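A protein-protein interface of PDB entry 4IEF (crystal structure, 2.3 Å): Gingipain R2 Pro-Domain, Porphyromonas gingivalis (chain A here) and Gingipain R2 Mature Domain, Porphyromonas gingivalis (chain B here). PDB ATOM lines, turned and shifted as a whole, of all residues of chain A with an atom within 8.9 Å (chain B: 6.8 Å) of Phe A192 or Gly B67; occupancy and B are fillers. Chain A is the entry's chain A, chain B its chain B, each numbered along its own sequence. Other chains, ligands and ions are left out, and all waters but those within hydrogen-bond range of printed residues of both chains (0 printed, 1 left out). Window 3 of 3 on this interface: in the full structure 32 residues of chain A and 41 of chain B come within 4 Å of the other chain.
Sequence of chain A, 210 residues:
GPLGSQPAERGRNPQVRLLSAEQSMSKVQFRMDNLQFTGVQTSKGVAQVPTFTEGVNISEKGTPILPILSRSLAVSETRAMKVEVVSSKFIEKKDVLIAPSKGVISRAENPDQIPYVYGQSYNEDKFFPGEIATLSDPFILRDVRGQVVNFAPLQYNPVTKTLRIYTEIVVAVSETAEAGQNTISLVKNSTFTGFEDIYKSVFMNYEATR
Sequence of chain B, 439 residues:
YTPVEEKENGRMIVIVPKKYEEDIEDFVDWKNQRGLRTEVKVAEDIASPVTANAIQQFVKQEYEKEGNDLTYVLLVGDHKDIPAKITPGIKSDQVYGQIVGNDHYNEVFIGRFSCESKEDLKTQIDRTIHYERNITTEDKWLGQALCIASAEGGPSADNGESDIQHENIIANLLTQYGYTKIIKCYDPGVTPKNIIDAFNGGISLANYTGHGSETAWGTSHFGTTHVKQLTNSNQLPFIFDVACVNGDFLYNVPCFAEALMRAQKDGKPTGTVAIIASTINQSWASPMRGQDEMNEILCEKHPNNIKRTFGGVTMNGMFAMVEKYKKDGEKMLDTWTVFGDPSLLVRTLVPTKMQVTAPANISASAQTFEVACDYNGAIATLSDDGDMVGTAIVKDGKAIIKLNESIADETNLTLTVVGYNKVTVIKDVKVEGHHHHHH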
ATOM      1  N   ARG A 142      15.023  -5.056  -5.233  1.00  0.00           N
ATOM      2  CA  ARG A 142      15.575  -3.700  -5.208  1.00  0.00           C
ATOM      3  C   ARG A 142      17.006  -3.680  -5.800  1.00  0.00           C
ATOM      4  O   ARG A 142      17.138  -3.613  -7.022  1.00  0.00           O
ATOM      5  CB  ARG A 142      15.500  -3.075  -3.799  1.00  0.00           C
ATOM      6  CG  ARG A 142      15.658  -1.568  -3.817  1.00  0.00           C
ATOM      7  CD  ARG A 142      14.992  -0.884  -2.658  1.00  0.00           C
ATOM      8  NE  ARG A 142      14.912   0.557  -2.895  1.00  0.00           N
ATOM      9  CZ  ARG A 142      13.784   1.254  -2.989  1.00  0.00           C
ATOM     10  NH1 ARG A 142      12.608   0.660  -2.817  1.00  0.00           N
ATOM     11  NH2 ARG A 142      13.822   2.557  -3.222  1.00  0.00           N
ATOM     12  N   ASP A 143      18.051  -3.758  -4.957  1.00  0.00           N
ATOM     13  CA  ASP A 143      19.447  -3.703  -5.399  1.00  0.00           C
ATOM     14  C   ASP A 143      20.159  -5.066  -5.308  1.00  0.00           C
ATOM     15  O   ASP A 143      21.357  -5.138  -5.590  1.00  0.00           O
ATOM     16  CB  ASP A 143      20.224  -2.651  -4.576  1.00  0.00           C
ATOM     17  CG  ASP A 143      19.687  -1.237  -4.695  1.00  0.00           C
ATOM     18  OD1 ASP A 143      19.308  -0.657  -3.653  1.00  0.00           O
ATOM     19  OD2 ASP A 143      19.656  -0.708  -5.823  1.00  0.00           O
ATOM     20  N   THR A 191      22.833   7.641  -0.536  1.00  0.00           N
ATOM     21  CA  THR A 191      22.342   6.330  -0.959  1.00  0.00           C
ATOM     22  C   THR A 191      21.236   5.837   0.002  1.00  0.00           C
ATOM     23  O   THR A 191      21.192   6.263   1.160  1.00  0.00           O
ATOM     24  CB  THR A 191      23.508   5.323  -1.098  1.00  0.00           C
ATOM     25  OG1 THR A 191      23.034   4.136  -1.732  1.00  0.00           O
ATOM     26  CG2 THR A 191      24.188   4.982   0.239  1.00  0.00           C
ATOM     27  N   PHE A 192      20.340   4.959  -0.495  1.00  0.00           N
ATOM     28  CA  PHE A 192      19.229   4.403   0.279  1.00  0.00           C
ATOM     29  C   PHE A 192      19.686   3.134   1.015  1.00  0.00           C
ATOM     30  O   PHE A 192      20.312   2.260   0.404  1.00  0.00           O
ATOM     31  CB  PHE A 192      18.023   4.130  -0.641  1.00  0.00           C
ATOM     32  CG  PHE A 192      16.807   3.517   0.018  1.00  0.00           C
ATOM     33  CD1 PHE A 192      16.021   4.256   0.896  1.00  0.00           C
ATOM     34  CD2 PHE A 192      16.423   2.217  -0.275  1.00  0.00           C
ATOM     35  CE1 PHE A 192      14.892   3.692   1.495  1.00  0.00           C
ATOM     36  CE2 PHE A 192      15.285   1.658   0.313  1.00  0.00           C
ATOM     37  CZ  PHE A 192      14.528   2.400   1.197  1.00  0.00           C
ATOM     38  N   THR A 193      19.377   3.046   2.328  1.00  0.00           N
ATOM     39  CA  THR A 193      19.797   1.947   3.210  1.00  0.00           C
ATOM     40  C   THR A 193      18.608   1.183   3.860  1.00  0.00           C
ATOM     41  O   THR A 193      18.836   0.217   4.585  1.00  0.00           O
ATOM     42  CB  THR A 193      20.760   2.514   4.293  1.00  0.00           C
ATOM     43  OG1 THR A 193      21.365   1.441   5.014  1.00  0.00           O
ATOM     44  CG2 THR A 193      20.083   3.488   5.262  1.00  0.00           C
ATOM     45  N   GLY A 194      17.380   1.617   3.582  1.00  0.00           N
ATOM     46  CA  GLY A 194      16.156   1.066   4.157  1.00  0.00           C
ATOM     47  C   GLY A 194      15.839  -0.396   3.910  1.00  0.00           C
ATOM     48  O   GLY A 194      15.085  -0.989   4.685  1.00  0.00           O
ATOM     49  N   PHE A 195      16.390  -0.992   2.839  1.00  0.00           N
ATOM     50  CA  PHE A 195      16.127  -2.393   2.496  1.00  0.00           C
ATOM     51  C   PHE A 195      17.188  -3.367   3.035  1.00  0.00           C
ATOM     52  O   PHE A 195      17.054  -4.570   2.812  1.00  0.00           O
ATOM     53  CB  PHE A 195      15.998  -2.550   0.973  1.00  0.00           C
ATOM     54  CG  PHE A 195      14.573  -2.574   0.469  1.00  0.00           C
ATOM     55  CD1 PHE A 195      14.053  -3.710  -0.138  1.00  0.00           C
ATOM     56  CD2 PHE A 195      13.752  -1.455   0.593  1.00  0.00           C
ATOM     57  CE1 PHE A 195      12.738  -3.730  -0.608  1.00  0.00           C
ATOM     58  CE2 PHE A 195      12.444  -1.470   0.110  1.00  0.00           C
ATOM     59  CZ  PHE A 195      11.940  -2.613  -0.476  1.00  0.00           C
ATOM     60  N   GLU A 196      18.211  -2.865   3.765  1.00  0.00           N
ATOM     61  CA  GLU A 196      19.293  -3.684   4.331  1.00  0.00           C
ATOM     62  C   GLU A 196      18.767  -4.783   5.252  1.00  0.00           C
ATOM     63  O   GLU A 196      19.185  -5.931   5.112  1.00  0.00           O
ATOM     64  CB  GLU A 196      20.322  -2.824   5.079  1.00  0.00           C
ATOM     65  CG  GLU A 196      21.224  -1.983   4.186  1.00  0.00           C
ATOM     66  CD  GLU A 196      22.063  -2.748   3.184  1.00  0.00           C
ATOM     67  OE1 GLU A 196      23.227  -3.068   3.512  1.00  0.00           O
ATOM     68  OE2 GLU A 196      21.569  -3.011   2.064  1.00  0.00           O
ATOM     69  N   ASP A 197      17.819  -4.448   6.150  1.00  0.00           N
ATOM     70  CA  ASP A 197      17.223  -5.412   7.075  1.00  0.00           C
ATOM     71  C   ASP A 197      16.295  -6.402   6.351  1.00  0.00           C
ATOM     72  O   ASP A 197      16.108  -7.520   6.836  1.00  0.00           O
ATOM     73  CB  ASP A 197      16.467  -4.704   8.202  1.00  0.00           C
ATOM     74  CG  ASP A 197      16.578  -5.451   9.512  1.00  0.00           C
ATOM     75  OD1 ASP A 197      17.621  -5.307  10.191  1.00  0.00           O
ATOM     76  OD2 ASP A 197      15.638  -6.196   9.849  1.00  0.00           O
ATOM     77  N   ILE A 198      15.729  -5.995   5.194  1.00  0.00           N
ATOM     78  CA  ILE A 198      14.879  -6.857   4.364  1.00  0.00           C
ATOM     79  C   ILE A 198      15.787  -7.926   3.727  1.00  0.00           C
ATOM     80  O   ILE A 198      15.446  -9.107   3.767  1.00  0.00           O
ATOM     81  CB  ILE A 198      14.072  -6.025   3.315  1.00  0.00           C
ATOM     82  CG1 ILE A 198      12.958  -5.209   4.007  1.00  0.00           C
ATOM     83  CG2 ILE A 198      13.499  -6.903   2.189  1.00  0.00           C
ATOM     84  CD1 ILE A 198      12.490  -3.998   3.247  1.00  0.00           C
ATOM     85  N   TYR A 199      16.959  -7.506   3.190  1.00  0.00           N
ATOM     86  CA  TYR A 199      17.940  -8.401   2.569  1.00  0.00           C
ATOM     87  C   TYR A 199      18.450  -9.446   3.563  1.00  0.00           C
ATOM     88  O   TYR A 199      18.613 -10.612   3.197  1.00  0.00           O
ATOM     89  CB  TYR A 199      19.141  -7.615   2.011  1.00  0.00           C
ATOM     90  CG  TYR A 199      18.847  -6.547   0.979  1.00  0.00           C
ATOM     91  CD1 TYR A 199      19.605  -5.382   0.923  1.00  0.00           C
ATOM     92  CD2 TYR A 199      17.871  -6.738   0.003  1.00  0.00           C
ATOM     93  CE1 TYR A 199      19.363  -4.407  -0.041  1.00  0.00           C
ATOM     94  CE2 TYR A 199      17.611  -5.765  -0.960  1.00  0.00           C
ATOM     95  CZ  TYR A 199      18.371  -4.607  -0.986  1.00  0.00           C
ATOM     96  OH  TYR A 199      18.148  -3.650  -1.944  1.00  0.00           O
ATOM     97  N   TYR A 206      23.248 -13.136   3.131  1.00  0.00           N
ATOM     98  CA  TYR A 206      23.463 -11.689   2.996  1.00  0.00           C
ATOM     99  C   TYR A 206      24.458 -11.125   4.027  1.00  0.00           C
ATOM    100  O   TYR A 206      25.392 -10.422   3.625  1.00  0.00           O
ATOM    101  CB  TYR A 206      22.139 -10.901   3.052  1.00  0.00           C
ATOM    102  CG  TYR A 206      22.312  -9.437   2.696  1.00  0.00           C
ATOM    103  CD1 TYR A 206      22.508  -9.038   1.376  1.00  0.00           C
ATOM    104  CD2 TYR A 206      22.323  -8.456   3.684  1.00  0.00           C
ATOM    105  CE1 TYR A 206      22.703  -7.697   1.048  1.00  0.00           C
ATOM    106  CE2 TYR A 206      22.516  -7.113   3.366  1.00  0.00           C
ATOM    107  CZ  TYR A 206      22.701  -6.737   2.046  1.00  0.00           C
ATOM    108  OH  TYR A 206      22.892  -5.414   1.725  1.00  0.00           O
ATOM    109  N   GLY B  10      13.022   6.550   3.429  1.00  0.00           N
ATOM    110  CA  GLY B  10      12.385   6.494   2.123  1.00  0.00           C
ATOM    111  C   GLY B  10      11.428   7.642   1.864  1.00  0.00           C
ATOM    112  O   GLY B  10      11.492   8.682   2.533  1.00  0.00           O
ATOM    113  N   ARG B  11      10.530   7.465   0.880  1.00  0.00           N
ATOM    114  CA  ARG B  11       9.561   8.491   0.508  1.00  0.00           C
ATOM    115  C   ARG B  11       8.306   7.882  -0.121  1.00  0.00           C
ATOM    116  O   ARG B  11       8.336   6.749  -0.600  1.00  0.00           O
ATOM    117  CB  ARG B  11      10.186   9.551  -0.423  1.00  0.00           C
ATOM    118  CG  ARG B  11      10.675   9.033  -1.770  1.00  0.00           C
ATOM    119  CD  ARG B  11      11.313  10.145  -2.575  1.00  0.00           C
ATOM    120  NE  ARG B  11      11.744   9.674  -3.890  1.00  0.00           N
ATOM    121  CZ  ARG B  11      11.033   9.809  -5.004  1.00  0.00           C
ATOM    122  NH1 ARG B  11       9.860  10.432  -4.981  1.00  0.00           N
ATOM    123  NH2 ARG B  11      11.497   9.337  -6.153  1.00  0.00           N
ATOM    124  N   TYR B  63      10.811   6.131  -9.461  1.00  0.00           N
ATOM    125  CA  TYR B  63      11.716   5.232  -8.738  1.00  0.00           C
ATOM    126  C   TYR B  63      13.171   5.509  -9.143  1.00  0.00           C
ATOM    127  O   TYR B  63      14.053   5.520  -8.284  1.00  0.00           O
ATOM    128  CB  TYR B  63      11.327   3.763  -9.027  1.00  0.00           C
ATOM    129  CG  TYR B  63      12.217   2.738  -8.361  1.00  0.00           C
ATOM    130  CD1 TYR B  63      11.896   2.210  -7.112  1.00  0.00           C
ATOM    131  CD2 TYR B  63      13.371   2.278  -8.987  1.00  0.00           C
ATOM    132  CE1 TYR B  63      12.727   1.282  -6.485  1.00  0.00           C
ATOM    133  CE2 TYR B  63      14.216   1.363  -8.365  1.00  0.00           C
ATOM    134  CZ  TYR B  63      13.877   0.849  -7.124  1.00  0.00           C
ATOM    135  OH  TYR B  63      14.690  -0.082  -6.528  1.00  0.00           O
ATOM    136  N   GLU B  64      13.401   5.762 -10.450  1.00  0.00           N
ATOM    137  CA  GLU B  64      14.712   6.008 -11.053  1.00  0.00           C
ATOM    138  C   GLU B  64      15.262   7.424 -10.775  1.00  0.00           C
ATOM    139  O   GLU B  64      16.405   7.706 -11.142  1.00  0.00           O
ATOM    140  CB  GLU B  64      14.652   5.741 -12.563  1.00  0.00           C
ATOM    141  CG  GLU B  64      14.623   4.254 -12.886  1.00  0.00           C
ATOM    142  CD  GLU B  64      14.068   3.822 -14.230  1.00  0.00           C
ATOM    143  OE1 GLU B  64      13.914   4.680 -15.130  1.00  0.00           O
ATOM    144  OE2 GLU B  64      13.799   2.608 -14.384  1.00  0.00           O
ATOM    145  N   LYS B  65      14.483   8.298 -10.104  1.00  0.00           N
ATOM    146  CA  LYS B  65      14.934   9.654  -9.765  1.00  0.00           C
ATOM    147  C   LYS B  65      15.985   9.620  -8.652  1.00  0.00           C
ATOM    148  O   LYS B  65      15.994   8.700  -7.830  1.00  0.00           O
ATOM    149  CB  LYS B  65      13.757  10.562  -9.365  1.00  0.00           C
ATOM    150  CG  LYS B  65      13.048  11.177 -10.566  1.00  0.00           C
ATOM    151  CD  LYS B  65      11.968  12.156 -10.166  1.00  0.00           C
ATOM    152  CE  LYS B  65      11.372  12.828 -11.380  1.00  0.00           C
ATOM    153  NZ  LYS B  65      10.209  13.687 -11.035  1.00  0.00           N
ATOM    154  N   GLU B  66      16.863  10.649  -8.645  1.00  0.00           N
ATOM    155  CA  GLU B  66      17.992  10.904  -7.737  1.00  0.00           C
ATOM    156  C   GLU B  66      17.762  10.382  -6.307  1.00  0.00           C
ATOM    157  O   GLU B  66      16.794  10.777  -5.651  1.00  0.00           O
ATOM    158  CB  GLU B  66      18.266  12.413  -7.690  1.00  0.00           C
ATOM    159  CG  GLU B  66      19.714  12.797  -7.434  1.00  0.00           C
ATOM    160  CD  GLU B  66      20.033  14.274  -7.594  1.00  0.00           C
ATOM    161  OE1 GLU B  66      19.149  15.041  -8.042  1.00  0.00           O
ATOM    162  OE2 GLU B  66      21.180  14.665  -7.280  1.00  0.00           O
ATOM    163  N   GLY B  67      18.640   9.484  -5.862  1.00  0.00           N
ATOM    164  CA  GLY B  67      18.580   8.922  -4.520  1.00  0.00           C
ATOM    165  C   GLY B  67      18.040   7.512  -4.418  1.00  0.00           C
ATOM    166  O   GLY B  67      18.344   6.824  -3.441  1.00  0.00           O
ATOM    167  N   ASN B  68      17.206   7.085  -5.409  1.00  0.00           N
ATOM    168  CA  ASN B  68      16.576   5.758  -5.502  1.00  0.00           C
ATOM    169  C   ASN B  68      15.922   5.378  -4.155  1.00  0.00           C
ATOM    170  O   ASN B  68      16.111   4.263  -3.661  1.00  0.00           O
ATOM    171  CB  ASN B  68      17.626   4.711  -5.939  1.00  0.00           C
ATOM    172  CG  ASN B  68      17.216   3.834  -7.098  1.00  0.00           C
ATOM    173  OD1 ASN B  68      17.025   2.621  -6.954  1.00  0.00           O
ATOM    174  ND2 ASN B  68      17.140   4.416  -8.286  1.00  0.00           N
ATOM    175  N   ASP B  69      15.168   6.325  -3.565  1.00  0.00           N
ATOM    176  CA  ASP B  69      14.561   6.202  -2.238  1.00  0.00           C
ATOM    177  C   ASP B  69      13.024   6.060  -2.242  1.00  0.00           C
ATOM    178  O   ASP B  69      12.428   6.049  -1.158  1.00  0.00           O
ATOM    179  CB  ASP B  69      14.969   7.414  -1.368  1.00  0.00           C
ATOM    180  CG  ASP B  69      14.561   8.775  -1.915  1.00  0.00           C
ATOM    181  OD1 ASP B  69      14.448   9.725  -1.112  1.00  0.00           O
ATOM    182  OD2 ASP B  69      14.345   8.887  -3.142  1.00  0.00           O
ATOM    183  N   LEU B  70      12.385   5.915  -3.427  1.00  0.00           N
ATOM    184  CA  LEU B  70      10.936   5.710  -3.502  1.00  0.00           C
ATOM    185  C   LEU B  70      10.593   4.372  -2.831  1.00  0.00           C
ATOM    186  O   LEU B  70      11.159   3.347  -3.206  1.00  0.00           O
ATOM    187  CB  LEU B  70      10.426   5.762  -4.958  1.00  0.00           C
ATOM    188  CG  LEU B  70       8.930   5.455  -5.183  1.00  0.00           C
ATOM    189  CD1 LEU B  70       8.028   6.448  -4.444  1.00  0.00           C
ATOM    190  CD2 LEU B  70       8.592   5.420  -6.667  1.00  0.00           C
ATOM    191  N   THR B  71       9.692   4.393  -1.822  1.00  0.00           N
ATOM    192  CA  THR B  71       9.346   3.194  -1.051  1.00  0.00           C
ATOM    193  C   THR B  71       7.826   2.929  -1.025  1.00  0.00           C
ATOM    194  O   THR B  71       7.415   1.767  -0.988  1.00  0.00           O
ATOM    195  CB  THR B  71       9.920   3.322   0.371  1.00  0.00           C
ATOM    196  OG1 THR B  71      11.314   3.596   0.273  1.00  0.00           O
ATOM    197  CG2 THR B  71       9.755   2.056   1.198  1.00  0.00           C
ATOM    198  N   GLU B 107       9.642  -3.683  -5.121  1.00  0.00           N
ATOM    199  CA  GLU B 107      10.637  -2.685  -4.734  1.00  0.00           C
ATOM    200  C   GLU B 107       9.936  -1.618  -3.903  1.00  0.00           C
ATOM    201  O   GLU B 107      10.517  -1.057  -2.972  1.00  0.00           O
ATOM    202  CB  GLU B 107      11.251  -2.032  -5.995  1.00  0.00           C
ATOM    203  CG  GLU B 107      12.331  -2.819  -6.706  1.00  0.00           C
ATOM    204  CD  GLU B 107      11.992  -4.209  -7.209  1.00  0.00           C
ATOM    205  OE1 GLU B 107      12.680  -5.151  -6.763  1.00  0.00           O
ATOM    206  OE2 GLU B 107      11.075  -4.366  -8.050  1.00  0.00           O
ATOM    207  N   ILE B 306      10.510   0.231   7.868  1.00  0.00           N
ATOM    208  CA  ILE B 306       9.689  -0.266   6.763  1.00  0.00           C
ATOM    209  C   ILE B 306       8.857  -1.474   7.255  1.00  0.00           C
ATOM    210  O   ILE B 306       7.657  -1.531   6.982  1.00  0.00           O
ATOM    211  CB  ILE B 306      10.571  -0.593   5.530  1.00  0.00           C
ATOM    212  CG1 ILE B 306      10.893   0.702   4.755  1.00  0.00           C
ATOM    213  CG2 ILE B 306       9.902  -1.618   4.625  1.00  0.00           C
ATOM    214  CD1 ILE B 306      12.069   0.623   3.792  1.00  0.00           C
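O of Asn B68 is in hydrogen-bond range of NH2 of Arg A142 (2.9 Å). The guanidinium group (NH2) of Arg A142 is in hydrogen-bond range of the backbone carbonyl oxygen (O) of Leu B70, at 2.8 Å. The guanidinium group of Arg A142 is in hydrogen-bond range of the backbone carbonyl oxygen of Glu B107 (2.7 Å).
The guanidinium group (NE) of Arg B11 lies within salt-bridge range of the side-chain carboxylate (OD2) of Asp B69 (2.8 Å). O of Arg B11 is in hydrogen-bond range of N of Thr B71 (3.0 Å). O of Tyr B63 is in hydrogen-bond range of ND2 of Asn B68. O of Asp B69 is in hydrogen-bond range of OG1 of Thr B71, at 3.1 Å.
OH of Tyr B63 touches CG of Arg A142, at 3.2 Å. Asp B69 touches Arg A142 (C to NH2, 3.7 Å). CA of Gly B10 touches CE1 of Phe A192, at 3.8 Å. Gly B67 touches Phe A192 (O to CB, 3.9 Å). O of Asn B68 touches CB of Phe A192 (3.6 Å). Asp B69 touches Phe A192 (CA to CD1, 3.97 Å). OG1 of Thr B71 touches CZ of Phe A192, 3.6 Å away. Gly A194 touches Ile B306. Phe A195 touches Glu B107 (CZ to O, 3.3 Å). CD1 of Ile A198 touches CG2 of Ile B306, at 3.8 Å.
Printed residues of chain B within 4 Å of Phe A192: Gly B10, Gly B67, Asn B68, Asp B69, Thr B71 and Ile B306. Of the printed residues of chain B, Ile A198 touches Ile B306. Printed residues of chain A within 4 Å of Gly B10: Phe A192. Glu B66 touches none of the printed residues of chain A. The nearest residue of chain A that does not touch Gly B67 is Thr A191 (4.6 Å).
Printed residues of chain B that touch a printed residue of chain A: Gly B10, Tyr B63, Gly B67, Asn B68, Asp B69, Leu B70, Thr B71, Glu B107 and Ile B306. Hydrophobic or aromatic side chains of chain A within 4 Å of the printed part of chain B: Phe A192, Phe A195 and Ile A198. Among the printed residues, 14 pairs touch across the chains. Among the printed residues, no Asp or Glu carboxylate lies within 4 Å of a Lys or Arg side-chain nitrogen of the other chain.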
